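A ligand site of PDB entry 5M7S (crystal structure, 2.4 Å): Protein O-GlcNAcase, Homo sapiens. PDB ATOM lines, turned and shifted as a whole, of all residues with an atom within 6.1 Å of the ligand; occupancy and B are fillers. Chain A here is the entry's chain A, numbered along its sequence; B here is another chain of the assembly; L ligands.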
ATOM      1  N   GLY A  67      12.229 -12.254  -8.634  1.00  0.00           N
ATOM      2  CA  GLY A  67      11.951 -10.820  -8.543  1.00  0.00           C
ATOM      3  C   GLY A  67      13.134  -9.901  -8.632  1.00  0.00           C
ATOM      4  O   GLY A  67      13.033  -8.744  -8.260  1.00  0.00           O
ATOM      5  N   PHE A  68      14.222 -10.378  -9.205  1.00  0.00           N
ATOM      6  CA  PHE A  68      15.510  -9.675  -9.099  1.00  0.00           C
ATOM      7  C   PHE A  68      15.817  -8.891 -10.364  1.00  0.00           C
ATOM      8  O   PHE A  68      15.136  -9.025 -11.367  1.00  0.00           O
ATOM      9  CB  PHE A  68      16.635 -10.654  -8.743  1.00  0.00           C
ATOM     10  CG  PHE A  68      16.640 -11.887  -9.559  1.00  0.00           C
ATOM     11  CD1 PHE A  68      17.093 -11.863 -10.849  1.00  0.00           C
ATOM     12  CD2 PHE A  68      16.193 -13.070  -9.050  1.00  0.00           C
ATOM     13  CE1 PHE A  68      17.073 -13.004 -11.648  1.00  0.00           C
ATOM     14  CE2 PHE A  68      16.163 -14.234  -9.829  1.00  0.00           C
ATOM     15  CZ  PHE A  68      16.613 -14.212 -11.133  1.00  0.00           C
ATOM     16  N   TYR A  69      16.834  -8.040 -10.291  1.00  0.00           N
ATOM     17  CA  TYR A  69      17.339  -7.312 -11.443  1.00  0.00           C
ATOM     18  C   TYR A  69      18.390  -8.158 -12.202  1.00  0.00           C
ATOM     19  O   TYR A  69      19.149  -8.893 -11.597  1.00  0.00           O
ATOM     20  CB  TYR A  69      17.972  -6.010 -10.980  1.00  0.00           C
ATOM     21  CG  TYR A  69      16.982  -4.945 -10.551  1.00  0.00           C
ATOM     22  CD1 TYR A  69      16.370  -4.123 -11.491  1.00  0.00           C
ATOM     23  CD2 TYR A  69      16.687  -4.701  -9.188  1.00  0.00           C
ATOM     24  CE1 TYR A  69      15.488  -3.125 -11.095  1.00  0.00           C
ATOM     25  CE2 TYR A  69      15.804  -3.722  -8.805  1.00  0.00           C
ATOM     26  CZ  TYR A  69      15.218  -2.928  -9.769  1.00  0.00           C
ATOM     27  OH  TYR A  69      14.348  -1.928  -9.442  1.00  0.00           O
ATOM     28  N   LYS A  98      12.372  -8.335 -12.990  1.00  0.00           N
ATOM     29  CA  LYS A  98      12.516  -6.924 -13.308  1.00  0.00           C
ATOM     30  C   LYS A  98      12.857  -6.557 -14.726  1.00  0.00           C
ATOM     31  O   LYS A  98      12.334  -5.544 -15.247  1.00  0.00           O
ATOM     32  CB  LYS A  98      13.538  -6.270 -12.382  1.00  0.00           C
ATOM     33  CG  LYS A  98      13.017  -6.041 -10.980  1.00  0.00           C
ATOM     34  CD  LYS A  98      12.060  -4.835 -10.925  1.00  0.00           C
ATOM     35  CE  LYS A  98      11.695  -4.434  -9.548  1.00  0.00           C
ATOM     36  NZ  LYS A  98      11.251  -5.594  -8.757  1.00  0.00           N
ATOM     37  N   ASP A 174       6.720  -1.266  -6.853  1.00  0.00           N
ATOM     38  CA  ASP A 174       7.994  -1.061  -6.200  1.00  0.00           C
ATOM     39  C   ASP A 174       8.990  -0.346  -7.100  1.00  0.00           C
ATOM     40  O   ASP A 174       8.964  -0.507  -8.296  1.00  0.00           O
ATOM     41  CB  ASP A 174       8.578  -2.393  -5.739  1.00  0.00           C
ATOM     42  CG  ASP A 174       8.702  -3.416  -6.854  1.00  0.00           C
ATOM     43  OD1 ASP A 174       7.801  -3.536  -7.749  1.00  0.00           O
ATOM     44  OD2 ASP A 174       9.720  -4.139  -6.778  1.00  0.00           O
ATOM     45  N   ASP A 175       9.883   0.432  -6.472  1.00  0.00           N
ATOM     46  CA  ASP A 175      11.031   1.038  -7.133  1.00  0.00           C
ATOM     47  C   ASP A 175      10.649   1.955  -8.289  1.00  0.00           C
ATOM     48  O   ASP A 175      11.182   1.863  -9.396  1.00  0.00           O
ATOM     49  CB  ASP A 175      12.023  -0.047  -7.610  1.00  0.00           C
ATOM     50  CG  ASP A 175      12.603  -0.904  -6.469  1.00  0.00           C
ATOM     51  OD1 ASP A 175      12.476  -0.567  -5.265  1.00  0.00           O
ATOM     52  OD2 ASP A 175      13.204  -1.952  -6.824  1.00  0.00           O
ATOM     53  N   CYS A 215       1.952  -5.038  -4.644  1.00  0.00           N
ATOM     54  CA  CYS A 215       3.203  -4.583  -4.028  1.00  0.00           C
ATOM     55  C   CYS A 215       3.213  -3.082  -3.857  1.00  0.00           C
ATOM     56  O   CYS A 215       3.184  -2.351  -4.842  1.00  0.00           O
ATOM     57  CB  CYS A 215       4.469  -5.022  -4.793  1.00  0.00           C
ATOM     58  SG  CYS A 215       5.962  -4.503  -3.867  1.00  0.00           S
ATOM     59  N   PRO A 216       3.278  -2.610  -2.610  1.00  0.00           N
ATOM     60  CA  PRO A 216       3.322  -1.169  -2.374  1.00  0.00           C
ATOM     61  C   PRO A 216       4.663  -0.536  -2.747  1.00  0.00           C
ATOM     62  O   PRO A 216       5.721  -1.208  -2.752  1.00  0.00           O
ATOM     63  CB  PRO A 216       3.121  -1.043  -0.874  1.00  0.00           C
ATOM     64  CG  PRO A 216       3.677  -2.307  -0.326  1.00  0.00           C
ATOM     65  CD  PRO A 216       3.500  -3.381  -1.380  1.00  0.00           C
ATOM     66  N   TYR A 219       7.322  -0.477   0.652  1.00  0.00           N
ATOM     67  CA  TYR A 219       7.323  -1.920   0.895  1.00  0.00           C
ATOM     68  C   TYR A 219       8.215  -2.458   2.017  1.00  0.00           C
ATOM     69  O   TYR A 219       8.382  -3.664   2.145  1.00  0.00           O
ATOM     70  CB  TYR A 219       7.698  -2.654  -0.368  1.00  0.00           C
ATOM     71  CG  TYR A 219       9.047  -2.355  -0.991  1.00  0.00           C
ATOM     72  CD1 TYR A 219      10.240  -2.870  -0.467  1.00  0.00           C
ATOM     73  CD2 TYR A 219       9.116  -1.619  -2.181  1.00  0.00           C
ATOM     74  CE1 TYR A 219      11.454  -2.634  -1.110  1.00  0.00           C
ATOM     75  CE2 TYR A 219      10.311  -1.397  -2.826  1.00  0.00           C
ATOM     76  CZ  TYR A 219      11.481  -1.909  -2.305  1.00  0.00           C
ATOM     77  OH  TYR A 219      12.663  -1.647  -2.950  1.00  0.00           O
ATOM     78  N   LEU A 248       2.383  -7.223  -0.296  1.00  0.00           N
ATOM     79  CA  LEU A 248       3.757  -7.697  -0.155  1.00  0.00           C
ATOM     80  C   LEU A 248       4.565  -6.728   0.699  1.00  0.00           C
ATOM     81  O   LEU A 248       4.318  -5.532   0.692  1.00  0.00           O
ATOM     82  CB  LEU A 248       4.391  -7.842  -1.527  1.00  0.00           C
ATOM     83  CG  LEU A 248       3.796  -8.945  -2.386  1.00  0.00           C
ATOM     84  CD1 LEU A 248       3.995  -8.590  -3.843  1.00  0.00           C
ATOM     85  CD2 LEU A 248       4.391 -10.307  -2.099  1.00  0.00           C
ATOM     86  N   TRP A 249       5.538  -7.260   1.443  1.00  0.00           N
ATOM     87  CA  TRP A 249       6.314  -6.500   2.421  1.00  0.00           C
ATOM     88  C   TRP A 249       7.655  -7.224   2.612  1.00  0.00           C
ATOM     89  O   TRP A 249       7.681  -8.439   2.621  1.00  0.00           O
ATOM     90  CB  TRP A 249       5.537  -6.481   3.731  1.00  0.00           C
ATOM     91  CG  TRP A 249       6.139  -5.726   4.875  1.00  0.00           C
ATOM     92  CD1 TRP A 249       6.693  -6.265   6.009  1.00  0.00           C
ATOM     93  CD2 TRP A 249       6.158  -4.311   5.053  1.00  0.00           C
ATOM     94  NE1 TRP A 249       7.092  -5.253   6.865  1.00  0.00           N
ATOM     95  CE2 TRP A 249       6.770  -4.047   6.305  1.00  0.00           C
ATOM     96  CE3 TRP A 249       5.730  -3.222   4.275  1.00  0.00           C
ATOM     97  CZ2 TRP A 249       6.974  -2.757   6.768  1.00  0.00           C
ATOM     98  CZ3 TRP A 249       5.922  -1.951   4.735  1.00  0.00           C
ATOM     99  CH2 TRP A 249       6.535  -1.722   5.976  1.00  0.00           C
ATOM    100  N   THR A 250       8.751  -6.486   2.774  1.00  0.00           N
ATOM    101  CA  THR A 250      10.090  -7.094   2.894  1.00  0.00           C
ATOM    102  C   THR A 250      10.707  -7.021   4.290  1.00  0.00           C
ATOM    103  O   THR A 250      11.856  -7.430   4.462  1.00  0.00           O
ATOM    104  CB  THR A 250      11.080  -6.462   1.903  1.00  0.00           C
ATOM    105  OG1 THR A 250      11.472  -5.170   2.358  1.00  0.00           O
ATOM    106  CG2 THR A 250      10.458  -6.329   0.529  1.00  0.00           C
ATOM    107  N   VAL A 254      14.847  -3.363   2.999  1.00  0.00           N
ATOM    108  CA  VAL A 254      14.832  -4.064   1.735  1.00  0.00           C
ATOM    109  C   VAL A 254      15.394  -5.482   1.956  1.00  0.00           C
ATOM    110  O   VAL A 254      14.744  -6.490   1.617  1.00  0.00           O
ATOM    111  CB  VAL A 254      15.664  -3.354   0.641  1.00  0.00           C
ATOM    112  CG1 VAL A 254      15.431  -4.057  -0.718  1.00  0.00           C
ATOM    113  CG2 VAL A 254      15.350  -1.855   0.573  1.00  0.00           C
ATOM    114  N   VAL A 255      16.582  -5.530   2.561  1.00  0.00           N
ATOM    115  CA  VAL A 255      17.211  -6.764   2.950  1.00  0.00           C
ATOM    116  C   VAL A 255      17.279  -6.818   4.451  1.00  0.00           C
ATOM    117  O   VAL A 255      18.192  -6.296   5.052  1.00  0.00           O
ATOM    118  CB  VAL A 255      18.634  -6.904   2.351  1.00  0.00           C
ATOM    119  CG1 VAL A 255      19.195  -8.291   2.663  1.00  0.00           C
ATOM    120  CG2 VAL A 255      18.630  -6.684   0.861  1.00  0.00           C
ATOM    121  N   TRP A 278       7.935 -10.794   0.941  1.00  0.00           N
ATOM    122  CA  TRP A 278       8.849 -10.933  -0.175  1.00  0.00           C
ATOM    123  C   TRP A 278      10.211 -10.778   0.477  1.00  0.00           C
ATOM    124  O   TRP A 278      10.639  -9.671   0.820  1.00  0.00           O
ATOM    125  CB  TRP A 278       8.582  -9.854  -1.216  1.00  0.00           C
ATOM    126  CG  TRP A 278       9.559  -9.667  -2.339  1.00  0.00           C
ATOM    127  CD1 TRP A 278      10.915  -9.613  -2.272  1.00  0.00           C
ATOM    128  CD2 TRP A 278       9.229  -9.397  -3.708  1.00  0.00           C
ATOM    129  NE1 TRP A 278      11.453  -9.378  -3.518  1.00  0.00           N
ATOM    130  CE2 TRP A 278      10.432  -9.225  -4.407  1.00  0.00           C
ATOM    131  CE3 TRP A 278       8.036  -9.311  -4.411  1.00  0.00           C
ATOM    132  CZ2 TRP A 278      10.466  -8.943  -5.752  1.00  0.00           C
ATOM    133  CZ3 TRP A 278       8.069  -9.051  -5.746  1.00  0.00           C
ATOM    134  CH2 TRP A 278       9.280  -8.858  -6.406  1.00  0.00           C
ATOM    135  N   ASN A 280      14.165 -10.859   0.846  1.00  0.00           N
ATOM    136  CA  ASN A 280      15.364 -10.613   0.073  1.00  0.00           C
ATOM    137  C   ASN A 280      16.647 -11.053   0.809  1.00  0.00           C
ATOM    138  O   ASN A 280      17.729 -10.708   0.389  1.00  0.00           O
ATOM    139  CB  ASN A 280      15.458  -9.121  -0.263  1.00  0.00           C
ATOM    140  CG  ASN A 280      14.347  -8.668  -1.208  1.00  0.00           C
ATOM    141  OD1 ASN A 280      14.182  -9.218  -2.285  1.00  0.00           O
ATOM    142  ND2 ASN A 280      13.613  -7.641  -0.798  1.00  0.00           N
ATOM    143  N   ALA A 283      18.967 -12.494  -1.756  1.00  0.00           N
ATOM    144  CA  ALA A 283      19.105 -11.748  -2.986  1.00  0.00           C
ATOM    145  C   ALA A 283      20.564 -11.281  -3.127  1.00  0.00           C
ATOM    146  O   ALA A 283      21.195 -10.927  -2.151  1.00  0.00           O
ATOM    147  CB  ALA A 283      18.157 -10.552  -2.983  1.00  0.00           C
ATOM    148  N   ASN A 284      21.070 -11.287  -4.353  1.00  0.00           N
ATOM    149  CA  ASN A 284      22.403 -10.825  -4.668  1.00  0.00           C
ATOM    150  C   ASN A 284      22.562  -9.979  -5.914  1.00  0.00           C
ATOM    151  O   ASN A 284      23.680  -9.820  -6.373  1.00  0.00           O
ATOM    152  CB  ASN A 284      23.363 -12.007  -4.720  1.00  0.00           C
ATOM    153  CG  ASN A 284      23.302 -12.797  -6.014  1.00  0.00           C
ATOM    154  OD1 ASN A 284      22.353 -12.691  -6.798  1.00  0.00           O
ATOM    155  ND2 ASN A 284      24.345 -13.588  -6.243  1.00  0.00           N
ATOM    156  N   ASP A 285      21.485  -9.361  -6.395  1.00  0.00           N
ATOM    157  CA  ASP A 285      21.541  -8.486  -7.583  1.00  0.00           C
ATOM    158  C   ASP A 285      22.131  -7.119  -7.328  1.00  0.00           C
ATOM    159  O   ASP A 285      22.357  -6.386  -8.270  1.00  0.00           O
ATOM    160  CB  ASP A 285      20.157  -8.301  -8.238  1.00  0.00           C
ATOM    161  CG  ASP A 285      19.051  -7.809  -7.261  1.00  0.00           C
ATOM    162  OD1 ASP A 285      19.365  -7.541  -6.057  1.00  0.00           O
ATOM    163  OD2 ASP A 285      17.875  -7.747  -7.710  1.00  0.00           O
ATOM    164  N   TYR A 286      22.415  -6.797  -6.071  1.00  0.00           N
ATOM    165  CA  TYR A 286      22.912  -5.473  -5.659  1.00  0.00           C
ATOM    166  C   TYR A 286      24.430  -5.352  -5.418  1.00  0.00           C
ATOM    167  O   TYR A 286      24.933  -4.256  -5.150  1.00  0.00           O
ATOM    168  CB  TYR A 286      22.208  -5.019  -4.391  1.00  0.00           C
ATOM    169  CG  TYR A 286      22.334  -5.921  -3.206  1.00  0.00           C
ATOM    170  CD1 TYR A 286      23.424  -5.848  -2.350  1.00  0.00           C
ATOM    171  CD2 TYR A 286      21.350  -6.842  -2.907  1.00  0.00           C
ATOM    172  CE1 TYR A 286      23.521  -6.646  -1.213  1.00  0.00           C
ATOM    173  CE2 TYR A 286      21.437  -7.654  -1.781  1.00  0.00           C
ATOM    174  CZ  TYR A 286      22.535  -7.541  -0.946  1.00  0.00           C
ATOM    175  OH  TYR A 286      22.611  -8.362   0.148  1.00  0.00           O
ATOM    176  N   ASN A 313      13.186 -14.220  -2.621  1.00  0.00           N
ATOM    177  CA  ASN A 313      13.729 -13.641  -3.861  1.00  0.00           C
ATOM    178  C   ASN A 313      15.234 -13.932  -3.792  1.00  0.00           C
ATOM    179  O   ASN A 313      15.973 -13.189  -3.183  1.00  0.00           O
ATOM    180  CB  ASN A 313      13.492 -12.129  -3.868  1.00  0.00           C
ATOM    181  CG  ASN A 313      13.985 -11.446  -5.137  1.00  0.00           C
ATOM    182  OD1 ASN A 313      13.736 -11.919  -6.217  1.00  0.00           O
ATOM    183  ND2 ASN A 313      14.627 -10.275  -4.997  1.00  0.00           N
ATOM    184  N   TRP B 679      23.735  -2.760   2.491  1.00  0.00           N
ATOM    185  CA  TRP B 679      24.854  -3.421   1.770  1.00  0.00           C
ATOM    186  C   TRP B 679      26.175  -2.662   2.090  1.00  0.00           C
ATOM    187  O   TRP B 679      26.788  -1.991   1.225  1.00  0.00           O
ATOM    188  CB  TRP B 679      24.558  -3.545   0.239  1.00  0.00           C
ATOM    189  CG  TRP B 679      23.854  -2.351  -0.457  1.00  0.00           C
ATOM    190  CD1 TRP B 679      24.465  -1.235  -0.938  1.00  0.00           C
ATOM    191  CD2 TRP B 679      22.435  -2.186  -0.758  1.00  0.00           C
ATOM    192  NE1 TRP B 679      23.528  -0.375  -1.500  1.00  0.00           N
ATOM    193  CE2 TRP B 679      22.279  -0.934  -1.398  1.00  0.00           C
ATOM    194  CE3 TRP B 679      21.284  -2.969  -0.538  1.00  0.00           C
ATOM    195  CZ2 TRP B 679      21.025  -0.453  -1.823  1.00  0.00           C
ATOM    196  CZ3 TRP B 679      20.038  -2.480  -0.944  1.00  0.00           C
ATOM    197  CH2 TRP B 679      19.923  -1.235  -1.592  1.00  0.00           C
HETATM  198  C1  LIG L   1      14.119  -4.626  -4.017  1.00  0.00           C
HETATM  199  C2  LIG L   1      13.714  -4.856  -5.482  1.00  0.00           C
HETATM  200  C3  LIG L   1      14.023  -6.248  -6.023  1.00  0.00           C
HETATM  201  C4  LIG L   1      15.473  -6.610  -5.685  1.00  0.00           C
HETATM  202  C5  LIG L   1      15.661  -6.522  -4.176  1.00  0.00           C
HETATM  203  C6  LIG L   1      17.059  -6.869  -3.718  1.00  0.00           C
HETATM  204  C7  LIG L   1      11.690  -4.898  -4.401  1.00  0.00           C
HETATM  205  C8  LIG L   1       9.181  -6.323  -2.694  1.00  0.00           C
HETATM  206  N1  LIG L   1      12.272  -4.530  -5.503  1.00  0.00           N
HETATM  207  O1  LIG L   1      13.807  -6.267  -7.445  1.00  0.00           O
HETATM  208  O2  LIG L   1      15.779  -7.936  -6.123  1.00  0.00           O
HETATM  209  O3  LIG L   1      15.391  -5.179  -3.719  1.00  0.00           O
HETATM  210  N2  LIG L   1      10.348  -4.878  -4.296  1.00  0.00           N
HETATM  211  O4  LIG L   1      18.021  -6.012  -4.341  1.00  0.00           O
HETATM  212  S1  LIG L   1      12.746  -5.360  -3.063  1.00  0.00           S
HETATM  213  C9  LIG L   1       9.599  -4.932  -3.051  1.00  0.00           C
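An oxygen (O2) of the ligand lies within hydrogen-bond range of the side-chain amide nitrogen of Asn 313, 2.8 Å away. An oxygen (O1) of the ligand sits at hydrogen-bond distance from the side-chain amino group of Lys 98 (3.0 Å). N2 of the ligand sits at hydrogen-bond distance from OD2 of Asp 174. OH of Tyr 219 sits close to S1 of the ligand (3.7 Å). An oxygen (O2) of the ligand is in hydrogen-bond range of the side-chain carboxylate (OD2) of Asp 285. The backbone carbonyl oxygen (O) of Gly 67 is in hydrogen-bond range of an oxygen (O1) of the ligand (2.7 Å). A sulfur (S1) of the ligand sits close to the side-chain amide nitrogen (ND2) of Asn 280, at 3.3 Å.
OD2 of Asp 175 lies close to N1 of the ligand, at 3.0 Å. Phe 68 touches the ligand (CA to O2, 3.5 Å). Tyr 69 touches the ligand. Cys 215 touches the ligand (SG to C9, 3.8 Å). Thr 250 touches the ligand (CG2 to C8, 3.5 Å). Val 254 touches the ligand (CG1 to O3, 3.2 Å). Trp 278 touches the ligand. Ala 283 touches the ligand (CB to C6, 3.9 Å). Tyr 286 touches the ligand (CD2 to O4, 3.7 Å). Hydrophobic or aromatic side chains within 4 Å of the ligand: Phe 68, Tyr 69, Tyr 219, Val 254, Trp 278, Ala 283 and Tyr 286. Along chain A the residues within 4 Å of the ligand span positions 67 to 313. The nearest printed residue that does not touch the ligand is Val 255 (4.8 Å).
The backbone NH of Tyr 69 sits at hydrogen-bond distance from the side-chain carboxylate of Asp 285, at 2.8 Å. The backbone carbonyl oxygen (O) of Trp 249 lies within hydrogen-bond range of the backbone NH (N) of Trp 278 (2.9 Å). The backbone NH (N) of Thr 250 sits at hydrogen-bond distance from the backbone carbonyl oxygen (O) of Tyr 219 (2.9 Å). OD1 of Asn 313 is in hydrogen-bond range of N of Phe 68 (3.4 Å). OD1 of Asp 175 lies within hydrogen-bond range of OH of Tyr 219 (2.6 Å). The backbone NH (N) of Gly 67 sits at hydrogen-bond distance from the side-chain amide oxygen (OD1) of Asn 313, 2.9 Å away. The side-chain carboxylate (OD2) of Asp 174 is in salt-bridge range of the side-chain amino group (NZ) of Lys 98 (2.9 Å). O of Asn 313 lies within hydrogen-bond range of N of Ala 283.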
